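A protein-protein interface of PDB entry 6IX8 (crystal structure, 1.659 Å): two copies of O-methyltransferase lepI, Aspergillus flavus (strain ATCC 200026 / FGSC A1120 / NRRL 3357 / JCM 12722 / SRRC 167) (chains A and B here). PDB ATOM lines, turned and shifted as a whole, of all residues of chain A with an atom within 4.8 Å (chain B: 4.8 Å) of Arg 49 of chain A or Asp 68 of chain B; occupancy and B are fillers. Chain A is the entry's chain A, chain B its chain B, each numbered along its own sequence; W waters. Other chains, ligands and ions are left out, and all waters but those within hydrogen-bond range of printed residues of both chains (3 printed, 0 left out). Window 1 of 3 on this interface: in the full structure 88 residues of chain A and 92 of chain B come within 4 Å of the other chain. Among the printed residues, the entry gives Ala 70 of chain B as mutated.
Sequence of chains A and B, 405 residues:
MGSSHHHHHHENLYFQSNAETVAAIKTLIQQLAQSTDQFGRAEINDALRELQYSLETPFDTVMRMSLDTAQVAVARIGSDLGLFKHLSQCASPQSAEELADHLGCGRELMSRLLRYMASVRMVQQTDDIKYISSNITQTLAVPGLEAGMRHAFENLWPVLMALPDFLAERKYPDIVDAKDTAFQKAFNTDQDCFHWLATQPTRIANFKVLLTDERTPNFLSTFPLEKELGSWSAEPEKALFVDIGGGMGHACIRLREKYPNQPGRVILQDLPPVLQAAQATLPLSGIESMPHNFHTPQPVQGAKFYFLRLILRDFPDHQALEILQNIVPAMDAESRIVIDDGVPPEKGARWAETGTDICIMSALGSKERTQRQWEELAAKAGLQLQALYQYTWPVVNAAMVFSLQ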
ATOM      1  N   ASN A  45      23.025  34.039 -16.263  1.00  0.00           N
ATOM      2  CA  ASN A  45      22.276  32.818 -16.568  1.00  0.00           C
ATOM      3  C   ASN A  45      20.782  33.067 -16.679  1.00  0.00           C
ATOM      4  O   ASN A  45      20.129  32.488 -17.547  1.00  0.00           O
ATOM      5  CB  ASN A  45      22.570  31.738 -15.544  1.00  0.00           C
ATOM      6  CG  ASN A  45      23.475  30.633 -16.182  1.00  0.00           C
ATOM      7  OD1 ASN A  45      24.326  30.954 -17.029  1.00  0.00           O
ATOM      8  ND2 ASN A  45      23.244  29.383 -15.865  1.00  0.00           N
ATOM      9  N   ASP A  46      20.227  33.901 -15.814  1.00  0.00           N
ATOM     10  CA  ASP A  46      18.812  34.248 -15.950  1.00  0.00           C
ATOM     11  C   ASP A  46      18.541  34.950 -17.269  1.00  0.00           C
ATOM     12  O   ASP A  46      17.510  34.714 -17.898  1.00  0.00           O
ATOM     13  CB  ASP A  46      18.407  35.173 -14.809  1.00  0.00           C
ATOM     14  CG  ASP A  46      17.435  34.508 -13.886  1.00  0.00           C
ATOM     15  OD1 ASP A  46      17.831  33.397 -13.392  1.00  0.00           O
ATOM     16  OD2 ASP A  46      16.282  35.044 -13.727  1.00  0.00           O
ATOM     17  N   ALA A  47      19.446  35.854 -17.686  1.00  0.00           N
ATOM     18  CA  ALA A  47      19.277  36.543 -18.959  1.00  0.00           C
ATOM     19  C   ALA A  47      19.301  35.553 -20.119  1.00  0.00           C
ATOM     20  O   ALA A  47      18.554  35.715 -21.091  1.00  0.00           O
ATOM     21  CB  ALA A  47      20.362  37.624 -19.113  1.00  0.00           C
ATOM     22  N   LEU A  48      20.165  34.535 -20.028  1.00  0.00           N
ATOM     23  CA  LEU A  48      20.290  33.550 -21.112  1.00  0.00           C
ATOM     24  C   LEU A  48      18.982  32.797 -21.234  1.00  0.00           C
ATOM     25  O   LEU A  48      18.509  32.535 -22.342  1.00  0.00           O
ATOM     26  CB  LEU A  48      21.428  32.546 -20.873  1.00  0.00           C
ATOM     27  CG  LEU A  48      22.855  33.164 -20.909  1.00  0.00           C
ATOM     28  CD1 LEU A  48      23.901  32.138 -20.500  1.00  0.00           C
ATOM     29  CD2 LEU A  48      23.135  33.706 -22.271  1.00  0.00           C
ATOM     30  N   ARG A  49      18.390  32.469 -20.095  1.00  0.00           N
ATOM     31  CA  ARG A  49      17.082  31.798 -20.103  1.00  0.00           C
ATOM     32  C   ARG A  49      15.991  32.712 -20.690  1.00  0.00           C
ATOM     33  O   ARG A  49      15.198  32.285 -21.540  1.00  0.00           O
ATOM     34  CB  ARG A  49      16.734  31.357 -18.668  1.00  0.00           C
ATOM     35  CG  ARG A  49      15.351  30.686 -18.623  1.00  0.00           C
ATOM     36  CD  ARG A  49      15.018  30.185 -17.205  1.00  0.00           C
ATOM     37  NE  ARG A  49      15.972  29.176 -16.725  1.00  0.00           N
ATOM     38  CZ  ARG A  49      15.613  28.050 -16.086  1.00  0.00           C
ATOM     39  NH1 ARG A  49      16.527  27.194 -15.636  1.00  0.00           N
ATOM     40  NH2 ARG A  49      14.341  27.812 -15.881  1.00  0.00           N
ATOM     41  N   GLU A  50      15.914  33.970 -20.220  1.00  0.00           N
ATOM     42  CA  GLU A  50      14.987  34.943 -20.790  1.00  0.00           C
ATOM     43  C   GLU A  50      15.149  35.078 -22.305  1.00  0.00           C
ATOM     44  O   GLU A  50      14.157  35.127 -23.053  1.00  0.00           O
ATOM     45  CB  GLU A  50      15.192  36.306 -20.133  1.00  0.00           C
ATOM     46  CG  GLU A  50      13.888  37.072 -20.217  1.00  0.00           C
ATOM     47  CD  GLU A  50      13.988  38.597 -20.231  1.00  0.00           C
ATOM     48  OE1 GLU A  50      15.077  39.175 -20.477  1.00  0.00           O
ATOM     49  OE2 GLU A  50      12.930  39.219 -19.953  1.00  0.00           O
ATOM     50  N   LEU A  51      16.389  35.112 -22.779  1.00  0.00           N
ATOM     51  CA  LEU A  51      16.618  35.207 -24.225  1.00  0.00           C
ATOM     52  C   LEU A  51      16.104  33.988 -24.955  1.00  0.00           C
ATOM     53  O   LEU A  51      15.456  34.118 -26.008  1.00  0.00           O
ATOM     54  CB  LEU A  51      18.117  35.373 -24.540  1.00  0.00           C
ATOM     55  CG  LEU A  51      18.579  36.803 -24.321  1.00  0.00           C
ATOM     56  CD1 LEU A  51      20.126  36.866 -24.230  1.00  0.00           C
ATOM     57  CD2 LEU A  51      18.048  37.700 -25.477  1.00  0.00           C
ATOM     58  N   GLN A  52      16.407  32.796 -24.426  1.00  0.00           N
ATOM     59  CA  GLN A  52      15.909  31.561 -25.031  1.00  0.00           C
ATOM     60  C   GLN A  52      14.389  31.623 -25.197  1.00  0.00           C
ATOM     61  O   GLN A  52      13.854  31.346 -26.297  1.00  0.00           O
ATOM     62  CB  GLN A  52      16.301  30.346 -24.176  1.00  0.00           C
ATOM     63  CG  GLN A  52      17.741  29.854 -24.351  1.00  0.00           C
ATOM     64  CD  GLN A  52      18.135  28.858 -23.249  1.00  0.00           C
ATOM     65  OE1 GLN A  52      18.837  29.208 -22.273  1.00  0.00           O
ATOM     66  NE2 GLN A  52      17.620  27.614 -23.371  1.00  0.00           N
ATOM     67  N   TYR A  53      13.680  32.002 -24.127  1.00  0.00           N
ATOM     68  CA  TYR A  53      12.217  31.992 -24.209  1.00  0.00           C
ATOM     69  C   TYR A  53      11.717  33.040 -25.172  1.00  0.00           C
ATOM     70  O   TYR A  53      10.710  32.811 -25.859  1.00  0.00           O
ATOM     71  CB  TYR A  53      11.556  32.243 -22.852  1.00  0.00           C
ATOM     72  CG  TYR A  53      11.770  31.142 -21.823  1.00  0.00           C
ATOM     73  CD1 TYR A  53      12.408  29.944 -22.154  1.00  0.00           C
ATOM     74  CD2 TYR A  53      11.470  31.377 -20.487  1.00  0.00           C
ATOM     75  CE1 TYR A  53      12.660  28.925 -21.167  1.00  0.00           C
ATOM     76  CE2 TYR A  53      11.660  30.362 -19.486  1.00  0.00           C
ATOM     77  CZ  TYR A  53      12.211  29.143 -19.830  1.00  0.00           C
ATOM     78  OH  TYR A  53      12.423  28.256 -18.796  1.00  0.00           O
ATOM     79  N   TRP A 351      12.234  33.042 -11.426  1.00  0.00           N
ATOM     80  CA  TRP A 351      11.571  31.734 -11.517  1.00  0.00           C
ATOM     81  C   TRP A 351      11.881  30.822 -10.319  1.00  0.00           C
ATOM     82  O   TRP A 351      11.043  29.986  -9.950  1.00  0.00           O
ATOM     83  CB  TRP A 351      11.937  30.994 -12.830  1.00  0.00           C
ATOM     84  CG  TRP A 351      13.392  30.665 -12.959  1.00  0.00           C
ATOM     85  CD1 TRP A 351      14.356  31.445 -13.559  1.00  0.00           C
ATOM     86  CD2 TRP A 351      14.075  29.466 -12.516  1.00  0.00           C
ATOM     87  NE1 TRP A 351      15.594  30.810 -13.475  1.00  0.00           N
ATOM     88  CE2 TRP A 351      15.426  29.610 -12.831  1.00  0.00           C
ATOM     89  CE3 TRP A 351      13.664  28.309 -11.821  1.00  0.00           C
ATOM     90  CZ2 TRP A 351      16.401  28.630 -12.474  1.00  0.00           C
ATOM     91  CZ3 TRP A 351      14.621  27.332 -11.506  1.00  0.00           C
ATOM     92  CH2 TRP A 351      15.966  27.502 -11.831  1.00  0.00           C
ATOM     93  N   GLN B  52      23.927  28.150 -20.625  1.00  0.00           N
ATOM     94  CA  GLN B  52      23.270  28.081 -19.334  1.00  0.00           C
ATOM     95  C   GLN B  52      23.748  26.855 -18.557  1.00  0.00           C
ATOM     96  O   GLN B  52      24.098  26.965 -17.368  1.00  0.00           O
ATOM     97  CB  GLN B  52      21.757  28.051 -19.538  1.00  0.00           C
ATOM     98  CG  GLN B  52      20.989  27.911 -18.264  1.00  0.00           C
ATOM     99  CD  GLN B  52      19.521  27.589 -18.517  1.00  0.00           C
ATOM    100  OE1 GLN B  52      18.836  26.985 -17.661  1.00  0.00           O
ATOM    101  NE2 GLN B  52      19.024  27.976 -19.703  1.00  0.00           N
ATOM    102  N   MET B  63      18.130  22.941  -8.795  1.00  0.00           N
ATOM    103  CA  MET B  63      16.941  23.777  -8.733  1.00  0.00           C
ATOM    104  C   MET B  63      16.225  23.760 -10.068  1.00  0.00           C
ATOM    105  O   MET B  63      14.989  23.725 -10.124  1.00  0.00           O
ATOM    106  CB  MET B  63      17.332  25.233  -8.385  1.00  0.00           C
ATOM    107  CG  MET B  63      17.687  25.465  -6.936  1.00  0.00           C
ATOM    108  SD  MET B  63      16.191  25.109  -5.940  1.00  0.00           S
ATOM    109  CE  MET B  63      15.090  26.341  -6.413  1.00  0.00           C
ATOM    110  N   ARG B  64      16.988  23.791 -11.173  1.00  0.00           N
ATOM    111  CA  ARG B  64      16.333  23.759 -12.481  1.00  0.00           C
ATOM    112  C   ARG B  64      15.643  22.411 -12.692  1.00  0.00           C
ATOM    113  O   ARG B  64      14.478  22.331 -13.142  1.00  0.00           O
ATOM    114  CB  ARG B  64      17.394  24.066 -13.541  1.00  0.00           C
ATOM    115  CG  ARG B  64      17.233  23.456 -14.856  1.00  0.00           C
ATOM    116  CD  ARG B  64      18.308  23.912 -15.800  1.00  0.00           C
ATOM    117  NE  ARG B  64      19.534  23.117 -15.809  1.00  0.00           N
ATOM    118  CZ  ARG B  64      19.651  21.844 -16.236  1.00  0.00           C
ATOM    119  NH1 ARG B  64      18.567  21.160 -16.736  1.00  0.00           N
ATOM    120  NH2 ARG B  64      20.834  21.264 -16.216  1.00  0.00           N
ATOM    121  N   MET B  65      16.334  21.310 -12.357  1.00  0.00           N
ATOM    122  CA  MET B  65      15.642  20.023 -12.464  1.00  0.00           C
ATOM    123  C   MET B  65      14.437  19.938 -11.512  1.00  0.00           C
ATOM    124  O   MET B  65      13.411  19.328 -11.852  1.00  0.00           O
ATOM    125  CB  MET B  65      16.638  18.859 -12.223  1.00  0.00           C
ATOM    126  CG  MET B  65      17.589  18.767 -13.409  1.00  0.00           C
ATOM    127  SD  MET B  65      18.712  17.331 -13.084  1.00  0.00           S
ATOM    128  CE  MET B  65      19.809  17.477 -14.504  1.00  0.00           C
ATOM    129  N   SER B  66      14.512  20.551 -10.333  1.00  0.00           N
ATOM    130  CA  SER B  66      13.392  20.481  -9.417  1.00  0.00           C
ATOM    131  C   SER B  66      12.205  21.271  -9.932  1.00  0.00           C
ATOM    132  O   SER B  66      11.063  20.895  -9.672  1.00  0.00           O
ATOM    133  CB  SER B  66      13.765  21.042  -8.054  1.00  0.00           C
ATOM    134  OG  SER B  66      14.776  20.258  -7.435  1.00  0.00           O
ATOM    135  N   LEU B  67      12.454  22.388 -10.605  1.00  0.00           N
ATOM    136  CA  LEU B  67      11.377  23.335 -10.854  1.00  0.00           C
ATOM    137  C   LEU B  67      10.920  23.430 -12.302  1.00  0.00           C
ATOM    138  O   LEU B  67       9.786  23.861 -12.532  1.00  0.00           O
ATOM    139  CB  LEU B  67      11.786  24.769 -10.383  1.00  0.00           C
ATOM    140  CG  LEU B  67      11.995  24.913  -8.879  1.00  0.00           C
ATOM    141  CD1 LEU B  67      12.318  26.384  -8.539  1.00  0.00           C
ATOM    142  CD2 LEU B  67      10.729  24.512  -8.152  1.00  0.00           C
ATOM    143  N   ASP B  68      11.726  23.126 -13.314  1.00  0.00           N
ATOM    144  CA  ASP B  68      11.276  23.440 -14.688  1.00  0.00           C
ATOM    145  C   ASP B  68      10.042  22.610 -15.062  1.00  0.00           C
ATOM    146  O   ASP B  68       9.221  23.044 -15.879  1.00  0.00           O
ATOM    147  CB  ASP B  68      12.422  23.201 -15.695  1.00  0.00           C
ATOM    148  CG  ASP B  68      13.465  24.353 -15.716  1.00  0.00           C
ATOM    149  OD1 ASP B  68      13.350  25.369 -14.970  1.00  0.00           O
ATOM    150  OD2 ASP B  68      14.445  24.192 -16.493  1.00  0.00           O
ATOM    151  N   THR B  69       9.939  21.426 -14.468  1.00  0.00           N
ATOM    152  CA  THR B  69       8.744  20.573 -14.400  1.00  0.00           C
ATOM    153  C   THR B  69       7.426  21.346 -14.242  1.00  0.00           C
ATOM    154  O   THR B  69       6.375  21.038 -14.854  1.00  0.00           O
ATOM    155  CB  THR B  69       8.940  19.705 -13.114  1.00  0.00           C
ATOM    156  OG1 THR B  69      10.193  18.982 -13.110  1.00  0.00           O
ATOM    157  CG2 THR B  69       7.755  18.778 -12.855  1.00  0.00           C
ATOM    158  N   ALA B  70       7.456  22.257 -13.292  1.00  0.00           N
ATOM    159  CA  ALA B  70       6.261  22.951 -12.874  1.00  0.00           C
ATOM    160  C   ALA B  70       5.667  23.730 -14.028  1.00  0.00           C
ATOM    161  O   ALA B  70       4.471  24.012 -14.025  1.00  0.00           O
ATOM    162  CB  ALA B  70       6.564  23.892 -11.725  1.00  0.00           C
ATOM    163  N   GLN B  71       6.467  24.088 -15.049  1.00  0.00           N
ATOM    164  CA  GLN B  71       5.859  24.874 -16.128  1.00  0.00           C
ATOM    165  C   GLN B  71       4.732  24.113 -16.825  1.00  0.00           C
ATOM    166  O   GLN B  71       3.738  24.735 -17.255  1.00  0.00           O
ATOM    167  CB  GLN B  71       6.889  25.269 -17.179  1.00  0.00           C
ATOM    168  CG  GLN B  71       7.993  26.207 -16.656  1.00  0.00           C
ATOM    169  CD  GLN B  71       8.830  26.824 -17.766  1.00  0.00           C
ATOM    170  OE1 GLN B  71       8.343  27.067 -18.874  1.00  0.00           O
ATOM    171  NE2 GLN B  71      10.095  27.097 -17.448  1.00  0.00           N
ATOM    172  N   VAL B  72       4.912  22.803 -17.039  1.00  0.00           N
ATOM    173  CA  VAL B  72       3.881  22.043 -17.742  1.00  0.00           C
ATOM    174  C   VAL B  72       2.579  22.010 -16.919  1.00  0.00           C
ATOM    175  O   VAL B  72       1.471  22.143 -17.470  1.00  0.00           O
ATOM    176  CB  VAL B  72       4.364  20.613 -18.057  1.00  0.00           C
ATOM    177  CG1 VAL B  72       3.288  19.878 -18.877  1.00  0.00           C
ATOM    178  CG2 VAL B  72       5.727  20.655 -18.841  1.00  0.00           C
HETATM  179  O   HOH W   1      12.472  29.309 -16.148  1.00  0.00           O
HETATM  180  O   HOH W   2      11.328  27.061 -14.759  1.00  0.00           O
HETATM  181  O   HOH W   3      16.116  25.762 -17.967  1.00  0.00           O
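The side-chain amide nitrogen of Asn 45 of chain A lies within hydrogen-bond range of the backbone carbonyl oxygen of Gln 52 of chain B, at 3.0 Å. The side-chain carboxylate (OD1) of Asp 68 of chain B lies within salt-bridge range of the guanidinium group (NH2) of Arg 49 of chain A, 2.8 Å away. OH of Tyr 53 of chain A lies within hydrogen-bond range of NE2 of Gln 71 of chain B (2.9 Å). The guanidinium group (NH1) of Arg 49 of chain A sits at hydrogen-bond distance from the side-chain amide oxygen (OE1) of Gln 52 of chain B, 3.1 Å away. OE1 of Gln 52 of chain A sits at hydrogen-bond distance from NE2 of Gln 52 of chain B (2.9 Å).
NE1 of Trp 351 of chain A lies within hydrogen-bond range of OD1 of Asp 46 of chain A (3.4 Å). OE1 of Gln 52 of chain A lies close to O of Leu 48 of chain A (3.3 Å).
Gln 52 of chain B touches Leu 48 of chain A (N to CD1, 3.99 Å). Arg 64 of chain B touches Arg 49 of chain A. Trp 351 of chain A touches Met 63 of chain B. CA of Arg 64 of chain B touches CH2 of Trp 351 of chain A, 3.8 Å away. Trp 351 of chain A touches Leu 67 of chain B.
Printed residues of chain B within 4 Å of Arg 49 of chain A: Gln 52 (3.1 Å), Arg 64 (3.7 Å) and Asp 68 (2.8 Å). Asp 68 of chain B touches just one residue of chain A: Arg 49. Of the printed residues of chain B, Trp 351 of chain A touches Met 63 (3.9 Å), Arg 64 (3.8 Å) and Leu 67 (3.9 Å). Of the printed residues of chain A, Gln 52 of chain B touches Asn 45 (3.0 Å), Leu 48 (3.99 Å), Arg 49 (3.1 Å) and Gln 52 (2.9 Å). Of the printed residues of chain B, Gln 52 of chain A touches Gln 52. Met 65 of chain B touches none of the printed residues of chain A. The nearest printed residue of chain B that does not touch Arg 49 of chain A is Gln 71 of chain B (4.6 Å).
Printed residues of chain B that touch a printed residue of chain A: Gln 52, Met 63, Arg 64, Leu 67, Asp 68 and Gln 71. Hydrophobic or aromatic side chains of chain B within 4 Å of the printed part of chain A: Leu 67. Of the 10 printed residues of chain A, 6 touch a printed residue of chain B. Printed residues of chain A that touch a printed residue of chain B: Asn 45, Leu 48, Arg 49, Gln 52, Tyr 53 and Trp 351. Hydrophobic or aromatic side chains of chain A within 4 Å of the printed part of chain B: Leu 48, Tyr 53 and Trp 351.
Gln 52 of chain B touches its own counterpart, Gln 52 of chain A. Of the 10 pairs that touch across the chains among the printed residues, 1 has its exchanged pair printed and touching as well.
Water W1 lies within hydrogen-bond range of the guanidinium group of Arg 49 of chain A (2.4 Å), the side-chain hydroxyl of Tyr 53 of chain A (2.9 Å) and the side-chain amide nitrogen of Gln 71 of chain B (3.5 Å). Water W2 lies within hydrogen-bond range of OD1 of Asp 68 of chain B, NE2 of Gln 71 of chain B and NH2 of Arg 49 of chain A. Water W3 lies within hydrogen-bond range of OD2 of Asp 68 of chain B (2.7 Å), NH1 of Arg 49 of chain A (2.8 Å) and OE1 of Gln 52 of chain B (3.0 Å).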
